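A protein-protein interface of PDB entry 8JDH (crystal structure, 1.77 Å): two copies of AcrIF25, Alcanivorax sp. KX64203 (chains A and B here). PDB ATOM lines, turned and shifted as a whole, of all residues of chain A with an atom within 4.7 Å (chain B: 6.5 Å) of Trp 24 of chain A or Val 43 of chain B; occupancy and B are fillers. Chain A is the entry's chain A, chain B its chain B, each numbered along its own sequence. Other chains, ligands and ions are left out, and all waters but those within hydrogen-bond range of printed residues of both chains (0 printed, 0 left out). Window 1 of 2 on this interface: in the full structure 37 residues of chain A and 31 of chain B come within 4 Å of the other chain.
Among the printed residues, merely in contact across the chains: Trp 24 of chain A with Val 43 of chain B (3.5 Å), Trp 24 of chain A with Glu 44 of chain B (3.5 Å), Val 43 of chain A with Trp 38 of chain B (3.5 Å), Trp 38 of chain A with Val 43 of chain B (3.6 Å), Val 20 of chain A with Glu 44 of chain B (3.6 Å), Trp 24 of chain A with Ile 12 of chain B (3.6 Å), Leu 35 of chain A with Ile 12 of chain B (3.7 Å), Val 16 of chain A with Ile 12 of chain B (3.8 Å), Lys 21 of chain A with Ile 12 of chain B (3.8 Å), Val 16 of chain A with Thr 40 of chain B (3.8 Å), Ile 39 of chain A with Val 43 of chain B (3.9 Å), Val 43 of chain A with Ile 39 of chain B (3.9 Å), Trp 24 of chain A with Thr 40 of chain B (3.9 Å) and Leu 14 of chain A with Ile 39 of chain B (3.9 Å).
Of the 16 printed residues of chain A, 11 touch a printed residue of chain B. Printed residues of chain A that touch a printed residue of chain B: Leu 14, Val 16, Val 20, Lys 21, Arg 23, Trp 24, Leu 35, Trp 38, Ile 39, Arg 42 and Val 43. Hydrophobic or aromatic side chains of chain A that line the printed part of chain B: Leu 14, Val 16, Val 20, Trp 24, Leu 35, Trp 38, Ile 39 and Val 43. Among the printed residues, Asp or Glu carboxylates within 4 Å of a Lys or Arg side-chain nitrogen of the other chain: Arg 23 of chain A with Glu 44 of chain B (2.7 Å).
Trp 38 of chain A touches Val 43 of chain B, and with the chains exchanged Val 43 of chain A touches Trp 38 of chain B. Ile 39 of chain A touches Val 43 of chain B, and with the chains exchanged Val 43 of chain A touches Ile 39 of chain B. Arg 42 of chain A touches its own counterpart, Arg 42 of chain B. Arg 42 of chain A touches Val 43 of chain B, and with the chains exchanged Val 43 of chain A touches Arg 42 of chain B. 4 positions are printed for both chains. Of the 19 pairs that touch across the chains among the printed residues, 7 have their exchanged pair printed and touching as well.
O of Trp 24 of chain A lies within hydrogen-bond range of OG of Ser 28 of chain A, 2.9 Å away.
NH2 of Arg 23 of chain A lies within salt-bridge range of OE2 of Glu 44 of chain B. O of Arg 42 of chain B sits close to O of Arg 42 of chain A. N of Ile 12 of chain B sits at hydrogen-bond distance from O of Leu 14 of chain A. The backbone carbonyl oxygen of Val 43 of chain B lies within hydrogen-bond range of the guanidinium group of Arg 42 of chain A (2.9 Å). O of Val 43 of chain A sits at hydrogen-bond distance from NH1 of Arg 42 of chain B (2.9 Å).
Of chain B, only Ile 12, Thr 40, Val 43 and Glu 44 come within 4 Å of Trp 24 of chain A. Of chain A, only Trp 24, Trp 38, Ile 39 and Arg 42 come within 4 Å of Val 43 of chain B. Printed residues of chain B within 4 Å of Val 20 of chain A: Glu 44 (3.6 Å). Of the printed residues of chain B, Val 16 of chain A touches Ile 12 and Thr 40. Of the printed residues of chain A, Glu 44 of chain B touches Val 20 (3.6 Å), Arg 23 (2.7 Å) and Trp 24 (3.5 Å). Printed residues of chain B within 4 Å of Trp 38 of chain A: Val 43 (3.6 Å). Gly 41 of chain B touches none of the printed residues of chain A.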
ATOM      1  N   LEU A  14      27.750  -3.429 -17.855  1.00  0.00           N
ATOM      2  CA  LEU A  14      28.639  -3.557 -16.708  1.00  0.00           C
ATOM      3  C   LEU A  14      28.471  -4.959 -16.131  1.00  0.00           C
ATOM      4  O   LEU A  14      27.393  -5.302 -15.635  1.00  0.00           O
ATOM      5  CB  LEU A  14      28.304  -2.480 -15.674  1.00  0.00           C
ATOM      6  CG  LEU A  14      29.203  -2.105 -14.497  1.00  0.00           C
ATOM      7  CD1 LEU A  14      30.526  -1.549 -14.977  1.00  0.00           C
ATOM      8  CD2 LEU A  14      28.486  -1.077 -13.626  1.00  0.00           C
ATOM      9  N   VAL A  16      29.577  -7.577 -13.309  1.00  0.00           N
ATOM     10  CA  VAL A  16      30.150  -7.670 -11.968  1.00  0.00           C
ATOM     11  C   VAL A  16      29.662  -8.946 -11.318  1.00  0.00           C
ATOM     12  O   VAL A  16      28.682  -9.565 -11.780  1.00  0.00           O
ATOM     13  CB  VAL A  16      29.782  -6.448 -11.095  1.00  0.00           C
ATOM     14  CG1 VAL A  16      30.458  -5.191 -11.621  1.00  0.00           C
ATOM     15  CG2 VAL A  16      28.269  -6.265 -11.037  1.00  0.00           C
ATOM     16  N   VAL A  20      28.237  -8.363  -5.798  1.00  0.00           N
ATOM     17  CA  VAL A  20      28.500  -6.928  -5.893  1.00  0.00           C
ATOM     18  C   VAL A  20      27.261  -6.195  -6.384  1.00  0.00           C
ATOM     19  O   VAL A  20      26.857  -5.165  -5.820  1.00  0.00           O
ATOM     20  CB  VAL A  20      29.702  -6.674  -6.823  1.00  0.00           C
ATOM     21  CG1 VAL A  20      29.889  -5.183  -7.059  1.00  0.00           C
ATOM     22  CG2 VAL A  20      30.974  -7.299  -6.244  1.00  0.00           C
ATOM     23  N   LYS A  21      26.639  -6.714  -7.450  1.00  0.00           N
ATOM     24  CA  LYS A  21      25.417  -6.098  -7.944  1.00  0.00           C
ATOM     25  C   LYS A  21      24.344  -6.089  -6.868  1.00  0.00           C
ATOM     26  O   LYS A  21      23.613  -5.107  -6.728  1.00  0.00           O
ATOM     27  CB  LYS A  21      24.897  -6.819  -9.187  1.00  0.00           C
ATOM     28  CG  LYS A  21      23.602  -6.212  -9.688  1.00  0.00           C
ATOM     29  CD  LYS A  21      23.063  -6.858 -10.957  1.00  0.00           C
ATOM     30  CE  LYS A  21      21.766  -6.179 -11.379  1.00  0.00           C
ATOM     31  NZ  LYS A  21      21.089  -6.887 -12.492  1.00  0.00           N
ATOM     32  N   GLY A  22      24.226  -7.178  -6.107  1.00  0.00           N
ATOM     33  CA  GLY A  22      23.221  -7.221  -5.059  1.00  0.00           C
ATOM     34  C   GLY A  22      23.440  -6.140  -4.021  1.00  0.00           C
ATOM     35  O   GLY A  22      22.491  -5.482  -3.582  1.00  0.00           O
ATOM     36  N   ARG A  23      24.699  -5.942  -3.626  1.00  0.00           N
ATOM     37  CA  ARG A  23      25.032  -4.906  -2.651  1.00  0.00           C
ATOM     38  C   ARG A  23      24.704  -3.516  -3.193  1.00  0.00           C
ATOM     39  O   ARG A  23      24.151  -2.670  -2.474  1.00  0.00           O
ATOM     40  CB  ARG A  23      26.515  -5.024  -2.290  1.00  0.00           C
ATOM     41  CG  ARG A  23      26.955  -4.200  -1.109  1.00  0.00           C
ATOM     42  CD  ARG A  23      28.351  -4.592  -0.599  1.00  0.00           C
ATOM     43  NE  ARG A  23      29.267  -5.072  -1.634  1.00  0.00           N
ATOM     44  CZ  ARG A  23      30.036  -4.282  -2.377  1.00  0.00           C
ATOM     45  NH1 ARG A  23      29.981  -2.965  -2.222  1.00  0.00           N
ATOM     46  NH2 ARG A  23      30.853  -4.804  -3.288  1.00  0.00           N
ATOM     47  N   TRP A  24      25.013  -3.272  -4.470  1.00  0.00           N
ATOM     48  CA  TRP A  24      24.705  -1.974  -5.062  1.00  0.00           C
ATOM     49  C   TRP A  24      23.205  -1.755  -5.181  1.00  0.00           C
ATOM     50  O   TRP A  24      22.709  -0.649  -4.939  1.00  0.00           O
ATOM     51  CB  TRP A  24      25.348  -1.856  -6.436  1.00  0.00           C
ATOM     52  CG  TRP A  24      26.837  -1.848  -6.420  1.00  0.00           C
ATOM     53  CD1 TRP A  24      27.662  -1.903  -5.334  1.00  0.00           C
ATOM     54  CD2 TRP A  24      27.683  -1.777  -7.568  1.00  0.00           C
ATOM     55  NE1 TRP A  24      28.983  -1.860  -5.741  1.00  0.00           N
ATOM     56  CE2 TRP A  24      29.017  -1.794  -7.111  1.00  0.00           C
ATOM     57  CE3 TRP A  24      27.439  -1.697  -8.942  1.00  0.00           C
ATOM     58  CZ2 TRP A  24      30.108  -1.725  -7.983  1.00  0.00           C
ATOM     59  CZ3 TRP A  24      28.520  -1.641  -9.809  1.00  0.00           C
ATOM     60  CH2 TRP A  24      29.837  -1.655  -9.325  1.00  0.00           C
ATOM     61  N   VAL A  25      22.468  -2.790  -5.586  1.00  0.00           N
ATOM     62  CA  VAL A  25      21.015  -2.672  -5.686  1.00  0.00           C
ATOM     63  C   VAL A  25      20.422  -2.372  -4.320  1.00  0.00           C
ATOM     64  O   VAL A  25      19.536  -1.516  -4.183  1.00  0.00           O
ATOM     65  CB  VAL A  25      20.410  -3.959  -6.289  1.00  0.00           C
ATOM     66  CG1 VAL A  25      18.887  -3.968  -6.127  1.00  0.00           C
ATOM     67  CG2 VAL A  25      20.765  -4.072  -7.766  1.00  0.00           C
ATOM     68  N   LYS A  26      20.920  -3.050  -3.288  1.00  0.00           N
ATOM     69  CA  LYS A  26      20.370  -2.853  -1.955  1.00  0.00           C
ATOM     70  C   LYS A  26      20.635  -1.438  -1.464  1.00  0.00           C
ATOM     71  O   LYS A  26      19.735  -0.789  -0.918  1.00  0.00           O
ATOM     72  CB  LYS A  26      20.952  -3.882  -0.987  1.00  0.00           C
ATOM     73  CG  LYS A  26      20.503  -3.707   0.461  1.00  0.00           C
ATOM     74  CD  LYS A  26      19.052  -4.129   0.661  1.00  0.00           C
ATOM     75  CE  LYS A  26      18.211  -3.026   1.317  1.00  0.00           C
ATOM     76  NZ  LYS A  26      17.700  -2.018   0.342  1.00  0.00           N
ATOM     77  N   GLU A  27      21.846  -0.922  -1.685  1.00  0.00           N
ATOM     78  CA  GLU A  27      22.113   0.427  -1.196  1.00  0.00           C
ATOM     79  C   GLU A  27      21.359   1.482  -1.997  1.00  0.00           C
ATOM     80  O   GLU A  27      20.800   2.418  -1.413  1.00  0.00           O
ATOM     81  CB  GLU A  27      23.611   0.728  -1.209  1.00  0.00           C
ATOM     82  CG  GLU A  27      23.939   2.132  -0.672  1.00  0.00           C
ATOM     83  CD  GLU A  27      23.446   2.352   0.765  1.00  0.00           C
ATOM     84  OE1 GLU A  27      23.314   1.363   1.517  1.00  0.00           O
ATOM     85  OE2 GLU A  27      23.168   3.513   1.144  1.00  0.00           O
ATOM     86  N   SER A  28      21.367   1.383  -3.333  1.00  0.00           N
ATOM     87  CA  SER A  28      20.563   2.287  -4.156  1.00  0.00           C
ATOM     88  C   SER A  28      19.101   2.292  -3.718  1.00  0.00           C
ATOM     89  O   SER A  28      18.478   3.355  -3.598  1.00  0.00           O
ATOM     90  CB  SER A  28      20.709   1.958  -5.646  1.00  0.00           C
ATOM     91  OG  SER A  28      20.354   0.626  -5.935  1.00  0.00           O
ATOM     92  N   LEU A  35      19.293   2.353  -9.717  1.00  0.00           N
ATOM     93  CA  LEU A  35      20.667   1.858  -9.697  1.00  0.00           C
ATOM     94  C   LEU A  35      21.568   2.664 -10.622  1.00  0.00           C
ATOM     95  O   LEU A  35      22.706   2.997 -10.257  1.00  0.00           O
ATOM     96  CB  LEU A  35      20.692   0.384 -10.100  1.00  0.00           C
ATOM     97  CG  LEU A  35      22.084  -0.240 -10.196  1.00  0.00           C
ATOM     98  CD1 LEU A  35      22.770  -0.186  -8.842  1.00  0.00           C
ATOM     99  CD2 LEU A  35      22.029  -1.671 -10.719  1.00  0.00           C
ATOM    100  N   TRP A  38      22.432   6.009  -9.093  1.00  0.00           N
ATOM    101  CA  TRP A  38      23.351   5.828  -7.971  1.00  0.00           C
ATOM    102  C   TRP A  38      24.780   5.612  -8.465  1.00  0.00           C
ATOM    103  O   TRP A  38      25.733   6.271  -8.006  1.00  0.00           O
ATOM    104  CB  TRP A  38      22.850   4.643  -7.140  1.00  0.00           C
ATOM    105  CG  TRP A  38      23.569   4.377  -5.872  1.00  0.00           C
ATOM    106  CD1 TRP A  38      23.360   4.974  -4.660  1.00  0.00           C
ATOM    107  CD2 TRP A  38      24.594   3.396  -5.668  1.00  0.00           C
ATOM    108  NE1 TRP A  38      24.205   4.432  -3.717  1.00  0.00           N
ATOM    109  CE2 TRP A  38      24.983   3.473  -4.312  1.00  0.00           C
ATOM    110  CE3 TRP A  38      25.231   2.473  -6.502  1.00  0.00           C
ATOM    111  CZ2 TRP A  38      25.978   2.653  -3.772  1.00  0.00           C
ATOM    112  CZ3 TRP A  38      26.217   1.655  -5.962  1.00  0.00           C
ATOM    113  CH2 TRP A  38      26.584   1.757  -4.614  1.00  0.00           C
ATOM    114  N   ILE A  39      24.938   4.704  -9.431  1.00  0.00           N
ATOM    115  CA  ILE A  39      26.253   4.439 -10.010  1.00  0.00           C
ATOM    116  C   ILE A  39      26.808   5.703 -10.655  1.00  0.00           C
ATOM    117  O   ILE A  39      27.973   6.071 -10.449  1.00  0.00           O
ATOM    118  CB  ILE A  39      26.163   3.282 -11.024  1.00  0.00           C
ATOM    119  CG1 ILE A  39      25.994   1.947 -10.294  1.00  0.00           C
ATOM    120  CG2 ILE A  39      27.392   3.244 -11.930  1.00  0.00           C
ATOM    121  CD1 ILE A  39      25.587   0.792 -11.220  1.00  0.00           C
ATOM    122  N   ARG A  42      28.129   8.207  -8.262  1.00  0.00           N
ATOM    123  CA  ARG A  42      29.404   7.896  -7.622  1.00  0.00           C
ATOM    124  C   ARG A  42      30.561   7.970  -8.607  1.00  0.00           C
ATOM    125  O   ARG A  42      31.664   8.360  -8.218  1.00  0.00           O
ATOM    126  CB  ARG A  42      29.369   6.511  -6.972  1.00  0.00           C
ATOM    127  CG  ARG A  42      28.628   6.491  -5.638  1.00  0.00           C
ATOM    128  CD  ARG A  42      28.845   5.178  -4.920  1.00  0.00           C
ATOM    129  NE  ARG A  42      28.309   5.208  -3.567  1.00  0.00           N
ATOM    130  CZ  ARG A  42      28.623   4.328  -2.624  1.00  0.00           C
ATOM    131  NH1 ARG A  42      29.481   3.346  -2.886  1.00  0.00           N
ATOM    132  NH2 ARG A  42      28.069   4.418  -1.423  1.00  0.00           N
ATOM    133  N   VAL A  43      30.313   7.728  -9.892  1.00  0.00           N
ATOM    134  CA  VAL A  43      31.393   7.863 -10.866  1.00  0.00           C
ATOM    135  C   VAL A  43      31.726   9.339 -11.064  1.00  0.00           C
ATOM    136  O   VAL A  43      32.896   9.734 -11.062  1.00  0.00           O
ATOM    137  CB  VAL A  43      31.012   7.199 -12.204  1.00  0.00           C
ATOM    138  CG1 VAL A  43      32.085   7.465 -13.264  1.00  0.00           C
ATOM    139  CG2 VAL A  43      30.804   5.703 -12.032  1.00  0.00           C
ATOM    140  N   ILE B  12      24.687  -5.361 -15.381  1.00  0.00           N
ATOM    141  CA  ILE B  12      24.037  -4.092 -15.076  1.00  0.00           C
ATOM    142  C   ILE B  12      23.923  -3.322 -16.382  1.00  0.00           C
ATOM    143  O   ILE B  12      24.900  -3.210 -17.133  1.00  0.00           O
ATOM    144  CB  ILE B  12      24.812  -3.280 -14.020  1.00  0.00           C
ATOM    145  CG1 ILE B  12      24.875  -4.037 -12.693  1.00  0.00           C
ATOM    146  CG2 ILE B  12      24.152  -1.928 -13.797  1.00  0.00           C
ATOM    147  CD1 ILE B  12      25.856  -3.460 -11.693  1.00  0.00           C
ATOM    148  N   TRP B  38      37.148   0.700 -14.536  1.00  0.00           N
ATOM    149  CA  TRP B  38      37.191   2.099 -14.133  1.00  0.00           C
ATOM    150  C   TRP B  38      35.917   2.484 -13.385  1.00  0.00           C
ATOM    151  O   TRP B  38      35.968   3.072 -12.290  1.00  0.00           O
ATOM    152  CB  TRP B  38      37.405   2.957 -15.381  1.00  0.00           C
ATOM    153  CG  TRP B  38      37.498   4.435 -15.170  1.00  0.00           C
ATOM    154  CD1 TRP B  38      38.603   5.149 -14.804  1.00  0.00           C
ATOM    155  CD2 TRP B  38      36.447   5.390 -15.354  1.00  0.00           C
ATOM    156  NE1 TRP B  38      38.299   6.489 -14.730  1.00  0.00           N
ATOM    157  CE2 TRP B  38      36.981   6.661 -15.060  1.00  0.00           C
ATOM    158  CE3 TRP B  38      35.098   5.290 -15.715  1.00  0.00           C
ATOM    159  CZ2 TRP B  38      36.218   7.822 -15.129  1.00  0.00           C
ATOM    160  CZ3 TRP B  38      34.341   6.448 -15.781  1.00  0.00           C
ATOM    161  CH2 TRP B  38      34.905   7.696 -15.491  1.00  0.00           C
ATOM    162  N   ILE B  39      34.758   2.111 -13.940  1.00  0.00           N
ATOM    163  CA  ILE B  39      33.489   2.412 -13.282  1.00  0.00           C
ATOM    164  C   ILE B  39      33.434   1.754 -11.910  1.00  0.00           C
ATOM    165  O   ILE B  39      33.140   2.411 -10.903  1.00  0.00           O
ATOM    166  CB  ILE B  39      32.298   1.968 -14.151  1.00  0.00           C
ATOM    167  CG1 ILE B  39      32.144   2.864 -15.379  1.00  0.00           C
ATOM    168  CG2 ILE B  39      31.012   2.008 -13.331  1.00  0.00           C
ATOM    169  CD1 ILE B  39      31.097   2.340 -16.397  1.00  0.00           C
ATOM    170  N   THR B  40      33.727   0.448 -11.848  1.00  0.00           N
ATOM    171  CA  THR B  40      33.650  -0.259 -10.574  1.00  0.00           C
ATOM    172  C   THR B  40      34.572   0.372  -9.542  1.00  0.00           C
ATOM    173  O   THR B  40      34.196   0.521  -8.373  1.00  0.00           O
ATOM    174  CB  THR B  40      33.976  -1.744 -10.759  1.00  0.00           C
ATOM    175  OG1 THR B  40      32.984  -2.340 -11.600  1.00  0.00           O
ATOM    176  CG2 THR B  40      33.966  -2.470  -9.421  1.00  0.00           C
ATOM    177  N   GLY B  41      35.784   0.754  -9.961  1.00  0.00           N
ATOM    178  CA  GLY B  41      36.731   1.379  -9.055  1.00  0.00           C
ATOM    179  C   GLY B  41      36.270   2.725  -8.546  1.00  0.00           C
ATOM    180  O   GLY B  41      36.766   3.203  -7.523  1.00  0.00           O
ATOM    181  N   ARG B  42      35.426   3.411  -9.314  1.00  0.00           N
ATOM    182  CA  ARG B  42      34.842   4.665  -8.848  1.00  0.00           C
ATOM    183  C   ARG B  42      33.574   4.485  -8.010  1.00  0.00           C
ATOM    184  O   ARG B  42      33.175   5.424  -7.317  1.00  0.00           O
ATOM    185  CB  ARG B  42      34.569   5.586 -10.038  1.00  0.00           C
ATOM    186  CG  ARG B  42      35.847   6.193 -10.610  1.00  0.00           C
ATOM    187  CD  ARG B  42      35.522   7.338 -11.555  1.00  0.00           C
ATOM    188  NE  ARG B  42      36.706   8.126 -11.881  1.00  0.00           N
ATOM    189  CZ  ARG B  42      36.665   9.400 -12.249  1.00  0.00           C
ATOM    190  NH1 ARG B  42      35.498  10.030 -12.336  1.00  0.00           N
ATOM    191  NH2 ARG B  42      37.790  10.041 -12.526  1.00  0.00           N
ATOM    192  N   VAL B  43      32.882   3.351  -8.126  1.00  0.00           N
ATOM    193  CA  VAL B  43      31.697   3.090  -7.303  1.00  0.00           C
ATOM    194  C   VAL B  43      32.078   2.590  -5.903  1.00  0.00           C
ATOM    195  O   VAL B  43      31.533   3.048  -4.889  1.00  0.00           O
ATOM    196  CB  VAL B  43      30.762   2.103  -8.025  1.00  0.00           C
ATOM    197  CG1 VAL B  43      29.614   1.666  -7.098  1.00  0.00           C
ATOM    198  CG2 VAL B  43      30.235   2.738  -9.316  1.00  0.00           C
ATOM    199  N   GLU B  44      33.002   1.635  -5.822  1.00  0.00           N
ATOM    200  CA  GLU B  44      33.365   1.055  -4.536  1.00  0.00           C
ATOM    201  C   GLU B  44      34.141   2.059  -3.679  1.00  0.00           C
ATOM    202  O   GLU B  44      34.702   3.041  -4.174  1.00  0.00           O
ATOM    203  CB  GLU B  44      34.192  -0.215  -4.745  1.00  0.00           C
ATOM    204  CG  GLU B  44      33.469  -1.328  -5.517  1.00  0.00           C
ATOM    205  CD  GLU B  44      32.448  -2.097  -4.674  1.00  0.00           C
ATOM    206  OE1 GLU B  44      31.946  -1.562  -3.664  1.00  0.00           O
ATOM    207  OE2 GLU B  44      32.139  -3.253  -5.025  1.00  0.00           O
ATOM    208  N   ALA B  45      34.163   1.806  -2.370  1.00  0.00           N
ATOM    209  CA  ALA B  45      34.813   2.714  -1.434  1.00  0.00           C
ATOM    210  C   ALA B  45      35.607   1.929  -0.393  1.00  0.00           C
ATOM    211  O   ALA B  45      35.501   2.167   0.809  1.00  0.00           O
ATOM    212  CB  ALA B  45      33.791   3.635  -0.768  1.00  0.00           C
